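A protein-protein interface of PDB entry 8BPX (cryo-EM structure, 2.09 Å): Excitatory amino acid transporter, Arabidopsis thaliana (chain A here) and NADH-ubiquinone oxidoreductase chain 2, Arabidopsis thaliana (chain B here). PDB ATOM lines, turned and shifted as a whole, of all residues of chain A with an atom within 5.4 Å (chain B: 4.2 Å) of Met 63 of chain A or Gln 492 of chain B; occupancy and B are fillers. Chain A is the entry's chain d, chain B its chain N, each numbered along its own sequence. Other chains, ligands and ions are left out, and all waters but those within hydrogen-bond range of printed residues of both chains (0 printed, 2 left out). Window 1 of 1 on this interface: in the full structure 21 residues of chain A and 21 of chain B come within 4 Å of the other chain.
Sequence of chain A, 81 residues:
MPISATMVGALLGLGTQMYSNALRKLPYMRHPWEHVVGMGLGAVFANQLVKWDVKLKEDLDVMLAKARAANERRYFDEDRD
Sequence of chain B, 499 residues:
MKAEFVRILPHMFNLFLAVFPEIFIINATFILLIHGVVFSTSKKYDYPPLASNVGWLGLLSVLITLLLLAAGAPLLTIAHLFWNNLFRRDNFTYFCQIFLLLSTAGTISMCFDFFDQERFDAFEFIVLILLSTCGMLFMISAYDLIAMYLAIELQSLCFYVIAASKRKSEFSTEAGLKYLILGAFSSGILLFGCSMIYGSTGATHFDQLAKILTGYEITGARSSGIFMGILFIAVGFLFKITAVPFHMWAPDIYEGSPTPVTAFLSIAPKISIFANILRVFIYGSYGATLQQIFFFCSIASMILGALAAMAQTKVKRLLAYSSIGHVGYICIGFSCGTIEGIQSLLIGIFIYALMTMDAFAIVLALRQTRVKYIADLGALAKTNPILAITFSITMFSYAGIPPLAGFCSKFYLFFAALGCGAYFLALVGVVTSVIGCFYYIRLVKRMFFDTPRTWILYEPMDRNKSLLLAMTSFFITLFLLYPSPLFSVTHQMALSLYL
OG of Ser 496 of chain B lies close to SD of Met 63 of chain A, 3.5 Å away.
The guanidinium group of Arg 68 of chain A lies within hydrogen-bond range of the backbone carbonyl oxygen of Leu 64 of chain A, 3.2 Å away.
The side-chain hydroxyl (OG) of Ser 496 of chain B sits at hydrogen-bond distance from the backbone carbonyl oxygen (O) of Gln 492 of chain B (2.8 Å).
Among the printed residues, pairs that only touch across the chains: Leu 56 of chain A with Gln 492 of chain B, Asp 59 of chain A with Gln 492 of chain B, Leu 60 of chain A with Leu 495 of chain B, Met 63 of chain A with Gln 492 of chain B, Met 63 of chain A with Leu 495 of chain B, Met 63 of chain A with Leu 499 of chain B, Leu 64 of chain A with His 491 of chain B, Leu 64 of chain A with Leu 495 of chain B and Ala 67 of chain A with Leu 499 of chain B.
Of the printed residues of chain B, Met 63 of chain A touches Gln 492, Leu 495, Ser 496 and Leu 499.
Of the printed residues of chain B, Leu 64 of chain A touches His 491 (3.8 Å) and Leu 495 (3.7 Å).
Printed residues of chain B within 4 Å of Asp 59 of chain A: Gln 492.
Of the printed residues of chain A, Leu 499 of chain B touches Met 63 and Ala 67.
Lys 66 of chain A touches none of the printed residues of chain B.
Val 489 of chain B touches none of the printed residues of chain A.
The nearest residue of chain A that does not touch Gln 492 of chain B is Leu 60 of chain A (4.04 Å).
Of the 11 printed residues of chain B, 5 touch a printed residue of chain A.
Hydrophobic or aromatic side chains of chain B that line the printed part of chain A: His 491, Leu 495 and Leu 499.
Among the printed residues, no Asp or Glu carboxylate lies within 4 Å of a Lys or Arg side-chain nitrogen of the other chain.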
ATOM      1  N   LEU A  56      -5.683 -29.294 -27.610  1.00  0.00           N
ATOM      2  CA  LEU A  56      -4.772 -28.530 -28.454  1.00  0.00           C
ATOM      3  C   LEU A  56      -5.329 -27.146 -28.751  1.00  0.00           C
ATOM      4  O   LEU A  56      -4.595 -26.152 -28.711  1.00  0.00           O
ATOM      5  CB  LEU A  56      -4.515 -29.281 -29.761  1.00  0.00           C
ATOM      6  CG  LEU A  56      -3.506 -30.430 -29.791  1.00  0.00           C
ATOM      7  CD1 LEU A  56      -3.579 -31.143 -31.132  1.00  0.00           C
ATOM      8  CD2 LEU A  56      -2.093 -29.933 -29.522  1.00  0.00           C
ATOM      9  N   ASP A  59      -4.879 -24.974 -25.639  1.00  0.00           N
ATOM     10  CA  ASP A  59      -3.534 -24.434 -25.431  1.00  0.00           C
ATOM     11  C   ASP A  59      -3.197 -23.359 -26.461  1.00  0.00           C
ATOM     12  O   ASP A  59      -2.594 -22.326 -26.121  1.00  0.00           O
ATOM     13  CB  ASP A  59      -2.492 -25.549 -25.461  1.00  0.00           C
ATOM     14  CG  ASP A  59      -2.874 -26.726 -24.594  1.00  0.00           C
ATOM     15  OD1 ASP A  59      -2.914 -27.854 -25.117  1.00  0.00           O
ATOM     16  OD2 ASP A  59      -3.141 -26.524 -23.392  1.00  0.00           O
ATOM     17  N   LEU A  60      -3.574 -23.583 -27.724  1.00  0.00           N
ATOM     18  CA  LEU A  60      -3.337 -22.574 -28.749  1.00  0.00           C
ATOM     19  C   LEU A  60      -4.031 -21.263 -28.415  1.00  0.00           C
ATOM     20  O   LEU A  60      -3.517 -20.191 -28.748  1.00  0.00           O
ATOM     21  CB  LEU A  60      -3.795 -23.079 -30.116  1.00  0.00           C
ATOM     22  CG  LEU A  60      -3.509 -22.123 -31.277  1.00  0.00           C
ATOM     23  CD1 LEU A  60      -2.031 -21.756 -31.322  1.00  0.00           C
ATOM     24  CD2 LEU A  60      -3.960 -22.706 -32.602  1.00  0.00           C
ATOM     25  N   ASP A  61      -5.192 -21.324 -27.758  1.00  0.00           N
ATOM     26  CA  ASP A  61      -5.892 -20.096 -27.389  1.00  0.00           C
ATOM     27  C   ASP A  61      -5.048 -19.231 -26.459  1.00  0.00           C
ATOM     28  O   ASP A  61      -4.834 -18.043 -26.725  1.00  0.00           O
ATOM     29  CB  ASP A  61      -7.231 -20.435 -26.741  1.00  0.00           C
ATOM     30  CG  ASP A  61      -8.261 -20.882 -27.753  1.00  0.00           C
ATOM     31  OD1 ASP A  61      -8.059 -20.615 -28.953  1.00  0.00           O
ATOM     32  OD2 ASP A  61      -9.263 -21.508 -27.350  1.00  0.00           O
ATOM     33  N   VAL A  62      -4.552 -19.817 -25.367  1.00  0.00           N
ATOM     34  CA  VAL A  62      -3.727 -19.068 -24.424  1.00  0.00           C
ATOM     35  C   VAL A  62      -2.465 -18.559 -25.104  1.00  0.00           C
ATOM     36  O   VAL A  62      -1.998 -17.442 -24.838  1.00  0.00           O
ATOM     37  CB  VAL A  62      -3.385 -19.941 -23.203  1.00  0.00           C
ATOM     38  CG1 VAL A  62      -2.807 -19.086 -22.091  1.00  0.00           C
ATOM     39  CG2 VAL A  62      -4.607 -20.708 -22.733  1.00  0.00           C
ATOM     40  N   MET A  63      -1.887 -19.373 -25.985  1.00  0.00           N
ATOM     41  CA  MET A  63      -0.614 -18.984 -26.578  1.00  0.00           C
ATOM     42  C   MET A  63      -0.799 -17.817 -27.547  1.00  0.00           C
ATOM     43  O   MET A  63       0.011 -16.879 -27.569  1.00  0.00           O
ATOM     44  CB  MET A  63       0.000 -20.199 -27.257  1.00  0.00           C
ATOM     45  CG  MET A  63       1.273 -20.656 -26.591  1.00  0.00           C
ATOM     46  SD  MET A  63       2.019 -22.031 -27.460  1.00  0.00           S
ATOM     47  CE  MET A  63       3.042 -21.114 -28.573  1.00  0.00           C
ATOM     48  N   LEU A  64      -1.878 -17.848 -28.336  1.00  0.00           N
ATOM     49  CA  LEU A  64      -2.237 -16.703 -29.167  1.00  0.00           C
ATOM     50  C   LEU A  64      -2.556 -15.480 -28.318  1.00  0.00           C
ATOM     51  O   LEU A  64      -2.266 -14.351 -28.718  1.00  0.00           O
ATOM     52  CB  LEU A  64      -3.428 -17.052 -30.059  1.00  0.00           C
ATOM     53  CG  LEU A  64      -3.209 -18.030 -31.212  1.00  0.00           C
ATOM     54  CD1 LEU A  64      -4.531 -18.565 -31.717  1.00  0.00           C
ATOM     55  CD2 LEU A  64      -2.467 -17.332 -32.334  1.00  0.00           C
ATOM     56  N   ALA A  65      -3.166 -15.685 -27.149  1.00  0.00           N
ATOM     57  CA  ALA A  65      -3.437 -14.559 -26.259  1.00  0.00           C
ATOM     58  C   ALA A  65      -2.143 -13.878 -25.837  1.00  0.00           C
ATOM     59  O   ALA A  65      -2.037 -12.644 -25.847  1.00  0.00           O
ATOM     60  CB  ALA A  65      -4.217 -15.032 -25.032  1.00  0.00           C
ATOM     61  N   LYS A  66      -1.141 -14.675 -25.461  1.00  0.00           N
ATOM     62  CA  LYS A  66       0.141 -14.100 -25.064  1.00  0.00           C
ATOM     63  C   LYS A  66       0.823 -13.402 -26.234  1.00  0.00           C
ATOM     64  O   LYS A  66       1.408 -12.324 -26.068  1.00  0.00           O
ATOM     65  CB  LYS A  66       1.053 -15.173 -24.478  1.00  0.00           C
ATOM     66  CG  LYS A  66       0.567 -15.740 -23.156  1.00  0.00           C
ATOM     67  CD  LYS A  66       1.487 -16.826 -22.608  1.00  0.00           C
ATOM     68  CE  LYS A  66       1.012 -17.376 -21.275  1.00  0.00           C
ATOM     69  NZ  LYS A  66       1.915 -18.449 -20.780  1.00  0.00           N
ATOM     70  N   ALA A  67       0.768 -14.004 -27.425  1.00  0.00           N
ATOM     71  CA  ALA A  67       1.333 -13.346 -28.600  1.00  0.00           C
ATOM     72  C   ALA A  67       0.662 -12.000 -28.851  1.00  0.00           C
ATOM     73  O   ALA A  67       1.338 -11.000 -29.129  1.00  0.00           O
ATOM     74  CB  ALA A  67       1.202 -14.248 -29.826  1.00  0.00           C
ATOM     75  N   ARG A  68      -0.669 -11.956 -28.748  1.00  0.00           N
ATOM     76  CA  ARG A  68      -1.401 -10.711 -28.957  1.00  0.00           C
ATOM     77  C   ARG A  68      -1.025  -9.663 -27.919  1.00  0.00           C
ATOM     78  O   ARG A  68      -0.880  -8.483 -28.250  1.00  0.00           O
ATOM     79  CB  ARG A  68      -2.906 -10.968 -28.918  1.00  0.00           C
ATOM     80  CG  ARG A  68      -3.578 -10.973 -30.278  1.00  0.00           C
ATOM     81  CD  ARG A  68      -4.965 -11.583 -30.187  1.00  0.00           C
ATOM     82  NE  ARG A  68      -4.911 -12.996 -29.823  1.00  0.00           N
ATOM     83  CZ  ARG A  68      -5.846 -13.624 -29.123  1.00  0.00           C
ATOM     84  NH1 ARG A  68      -6.924 -12.994 -28.687  1.00  0.00           N
ATOM     85  NH2 ARG A  68      -5.695 -14.916 -28.853  1.00  0.00           N
ATOM     86  N   PHE B  95       7.340 -31.747 -29.363  1.00  0.00           N
ATOM     87  CA  PHE B  95       6.611 -32.351 -30.508  1.00  0.00           C
ATOM     88  C   PHE B  95       7.603 -32.865 -31.567  1.00  0.00           C
ATOM     89  O   PHE B  95       7.349 -33.927 -32.133  1.00  0.00           O
ATOM     90  CB  PHE B  95       5.604 -31.357 -31.098  1.00  0.00           C
ATOM     91  CG  PHE B  95       4.425 -31.080 -30.200  1.00  0.00           C
ATOM     92  CD1 PHE B  95       3.561 -32.099 -29.830  1.00  0.00           C
ATOM     93  CD2 PHE B  95       4.184 -29.805 -29.712  1.00  0.00           C
ATOM     94  CE1 PHE B  95       2.480 -31.847 -29.000  1.00  0.00           C
ATOM     95  CE2 PHE B  95       3.101 -29.555 -28.883  1.00  0.00           C
ATOM     96  CZ  PHE B  95       2.250 -30.576 -28.529  1.00  0.00           C
ATOM     97  N   SER B 488      -3.479 -27.283 -35.544  1.00  0.00           N
ATOM     98  CA  SER B 488      -3.341 -26.682 -34.222  1.00  0.00           C
ATOM     99  C   SER B 488      -1.964 -26.946 -33.625  1.00  0.00           C
ATOM    100  O   SER B 488      -1.343 -26.034 -33.071  1.00  0.00           O
ATOM    101  CB  SER B 488      -4.436 -27.201 -33.294  1.00  0.00           C
ATOM    102  OG  SER B 488      -5.707 -27.074 -33.900  1.00  0.00           O
ATOM    103  N   VAL B 489      -1.492 -28.192 -33.748  1.00  0.00           N
ATOM    104  CA  VAL B 489      -0.210 -28.601 -33.098  1.00  0.00           C
ATOM    105  C   VAL B 489       0.950 -27.834 -33.751  1.00  0.00           C
ATOM    106  O   VAL B 489       1.881 -27.470 -33.027  1.00  0.00           O
ATOM    107  CB  VAL B 489       0.013 -30.131 -33.096  1.00  0.00           C
ATOM    108  CG1 VAL B 489       0.447 -30.677 -34.445  1.00  0.00           C
ATOM    109  CG2 VAL B 489       0.994 -30.551 -32.017  1.00  0.00           C
ATOM    110  N   THR B 490       0.860 -27.574 -35.053  1.00  0.00           N
ATOM    111  CA  THR B 490       1.940 -26.912 -35.829  1.00  0.00           C
ATOM    112  C   THR B 490       1.883 -25.393 -35.631  1.00  0.00           C
ATOM    113  O   THR B 490       2.954 -24.776 -35.627  1.00  0.00           O
ATOM    114  CB  THR B 490       1.888 -27.255 -37.322  1.00  0.00           C
ATOM    115  OG1 THR B 490       0.571 -27.036 -37.827  1.00  0.00           O
ATOM    116  CG2 THR B 490       2.326 -28.677 -37.603  1.00  0.00           C
ATOM    117  N   HIS B 491       0.683 -24.829 -35.487  1.00  0.00           N
ATOM    118  CA  HIS B 491       0.595 -23.431 -35.074  1.00  0.00           C
ATOM    119  C   HIS B 491       1.181 -23.240 -33.681  1.00  0.00           C
ATOM    120  O   HIS B 491       1.917 -22.275 -33.428  1.00  0.00           O
ATOM    121  CB  HIS B 491      -0.858 -22.960 -35.118  1.00  0.00           C
ATOM    122  CG  HIS B 491      -1.014 -21.475 -35.243  1.00  0.00           C
ATOM    123  ND1 HIS B 491      -2.071 -20.892 -35.905  1.00  0.00           N
ATOM    124  CD2 HIS B 491      -0.250 -20.457 -34.781  1.00  0.00           C
ATOM    125  CE1 HIS B 491      -1.950 -19.577 -35.851  1.00  0.00           C
ATOM    126  NE2 HIS B 491      -0.854 -19.288 -35.174  1.00  0.00           N
ATOM    127  N   GLN B 492       0.870 -24.165 -32.771  1.00  0.00           N
ATOM    128  CA  GLN B 492       1.451 -24.156 -31.434  1.00  0.00           C
ATOM    129  C   GLN B 492       2.973 -24.150 -31.490  1.00  0.00           C
ATOM    130  O   GLN B 492       3.626 -23.334 -30.835  1.00  0.00           O
ATOM    131  CB  GLN B 492       0.950 -25.374 -30.661  1.00  0.00           C
ATOM    132  CG  GLN B 492       1.208 -25.346 -29.181  1.00  0.00           C
ATOM    133  CD  GLN B 492       0.375 -26.373 -28.438  1.00  0.00           C
ATOM    134  OE1 GLN B 492      -0.814 -26.537 -28.708  1.00  0.00           O
ATOM    135  NE2 GLN B 492       0.998 -27.069 -27.498  1.00  0.00           N
ATOM    136  N   MET B 493       3.540 -25.055 -32.280  1.00  0.00           N
ATOM    137  CA  MET B 493       5.013 -25.194 -32.379  1.00  0.00           C
ATOM    138  C   MET B 493       5.620 -23.904 -32.948  1.00  0.00           C
ATOM    139  O   MET B 493       6.636 -23.458 -32.408  1.00  0.00           O
ATOM    140  CB  MET B 493       5.358 -26.379 -33.283  1.00  0.00           C
ATOM    141  CG  MET B 493       5.041 -27.709 -32.641  1.00  0.00           C
ATOM    142  SD  MET B 493       5.121 -29.063 -33.824  1.00  0.00           S
ATOM    143  CE  MET B 493       6.897 -29.216 -33.999  1.00  0.00           C
ATOM    144  N   ALA B 494       5.018 -23.350 -34.005  1.00  0.00           N
ATOM    145  CA  ALA B 494       5.552 -22.134 -34.682  1.00  0.00           C
ATOM    146  C   ALA B 494       5.612 -20.990 -33.657  1.00  0.00           C
ATOM    147  O   ALA B 494       6.640 -20.358 -33.576  1.00  0.00           O
ATOM    148  CB  ALA B 494       4.777 -21.736 -35.904  1.00  0.00           C
ATOM    149  N   LEU B 495       4.553 -20.820 -32.905  1.00  0.00           N
ATOM    150  CA  LEU B 495       4.513 -19.797 -31.829  1.00  0.00           C
ATOM    151  C   LEU B 495       5.535 -20.047 -30.749  1.00  0.00           C
ATOM    152  O   LEU B 495       6.140 -19.081 -30.363  1.00  0.00           O
ATOM    153  CB  LEU B 495       3.096 -19.660 -31.271  1.00  0.00           C
ATOM    154  CG  LEU B 495       2.114 -18.945 -32.196  1.00  0.00           C
ATOM    155  CD1 LEU B 495       0.720 -18.959 -31.599  1.00  0.00           C
ATOM    156  CD2 LEU B 495       2.562 -17.513 -32.454  1.00  0.00           C
ATOM    157  N   SER B 496       5.732 -21.296 -30.302  1.00  0.00           N
ATOM    158  CA  SER B 496       6.649 -21.629 -29.186  1.00  0.00           C
ATOM    159  C   SER B 496       8.119 -21.284 -29.488  1.00  0.00           C
ATOM    160  O   SER B 496       8.832 -21.096 -28.532  1.00  0.00           O
ATOM    161  CB  SER B 496       6.471 -23.098 -28.756  1.00  0.00           C
ATOM    162  OG  SER B 496       5.122 -23.405 -28.465  1.00  0.00           O
ATOM    163  N   LEU B 499       7.959 -17.742 -28.069  1.00  0.00           N
ATOM    164  CA  LEU B 499       7.024 -17.490 -26.950  1.00  0.00           C
ATOM    165  C   LEU B 499       6.323 -18.762 -26.566  1.00  0.00           C
ATOM    166  O   LEU B 499       6.053 -18.940 -25.351  1.00  0.00           O
ATOM    167  CB  LEU B 499       5.940 -16.492 -27.456  1.00  0.00           C
ATOM    168  CG  LEU B 499       4.869 -17.051 -28.387  1.00  0.00           C
ATOM    169  CD1 LEU B 499       3.571 -17.325 -27.644  1.00  0.00           C
ATOM    170  CD2 LEU B 499       4.622 -16.099 -29.546  1.00  0.00           C
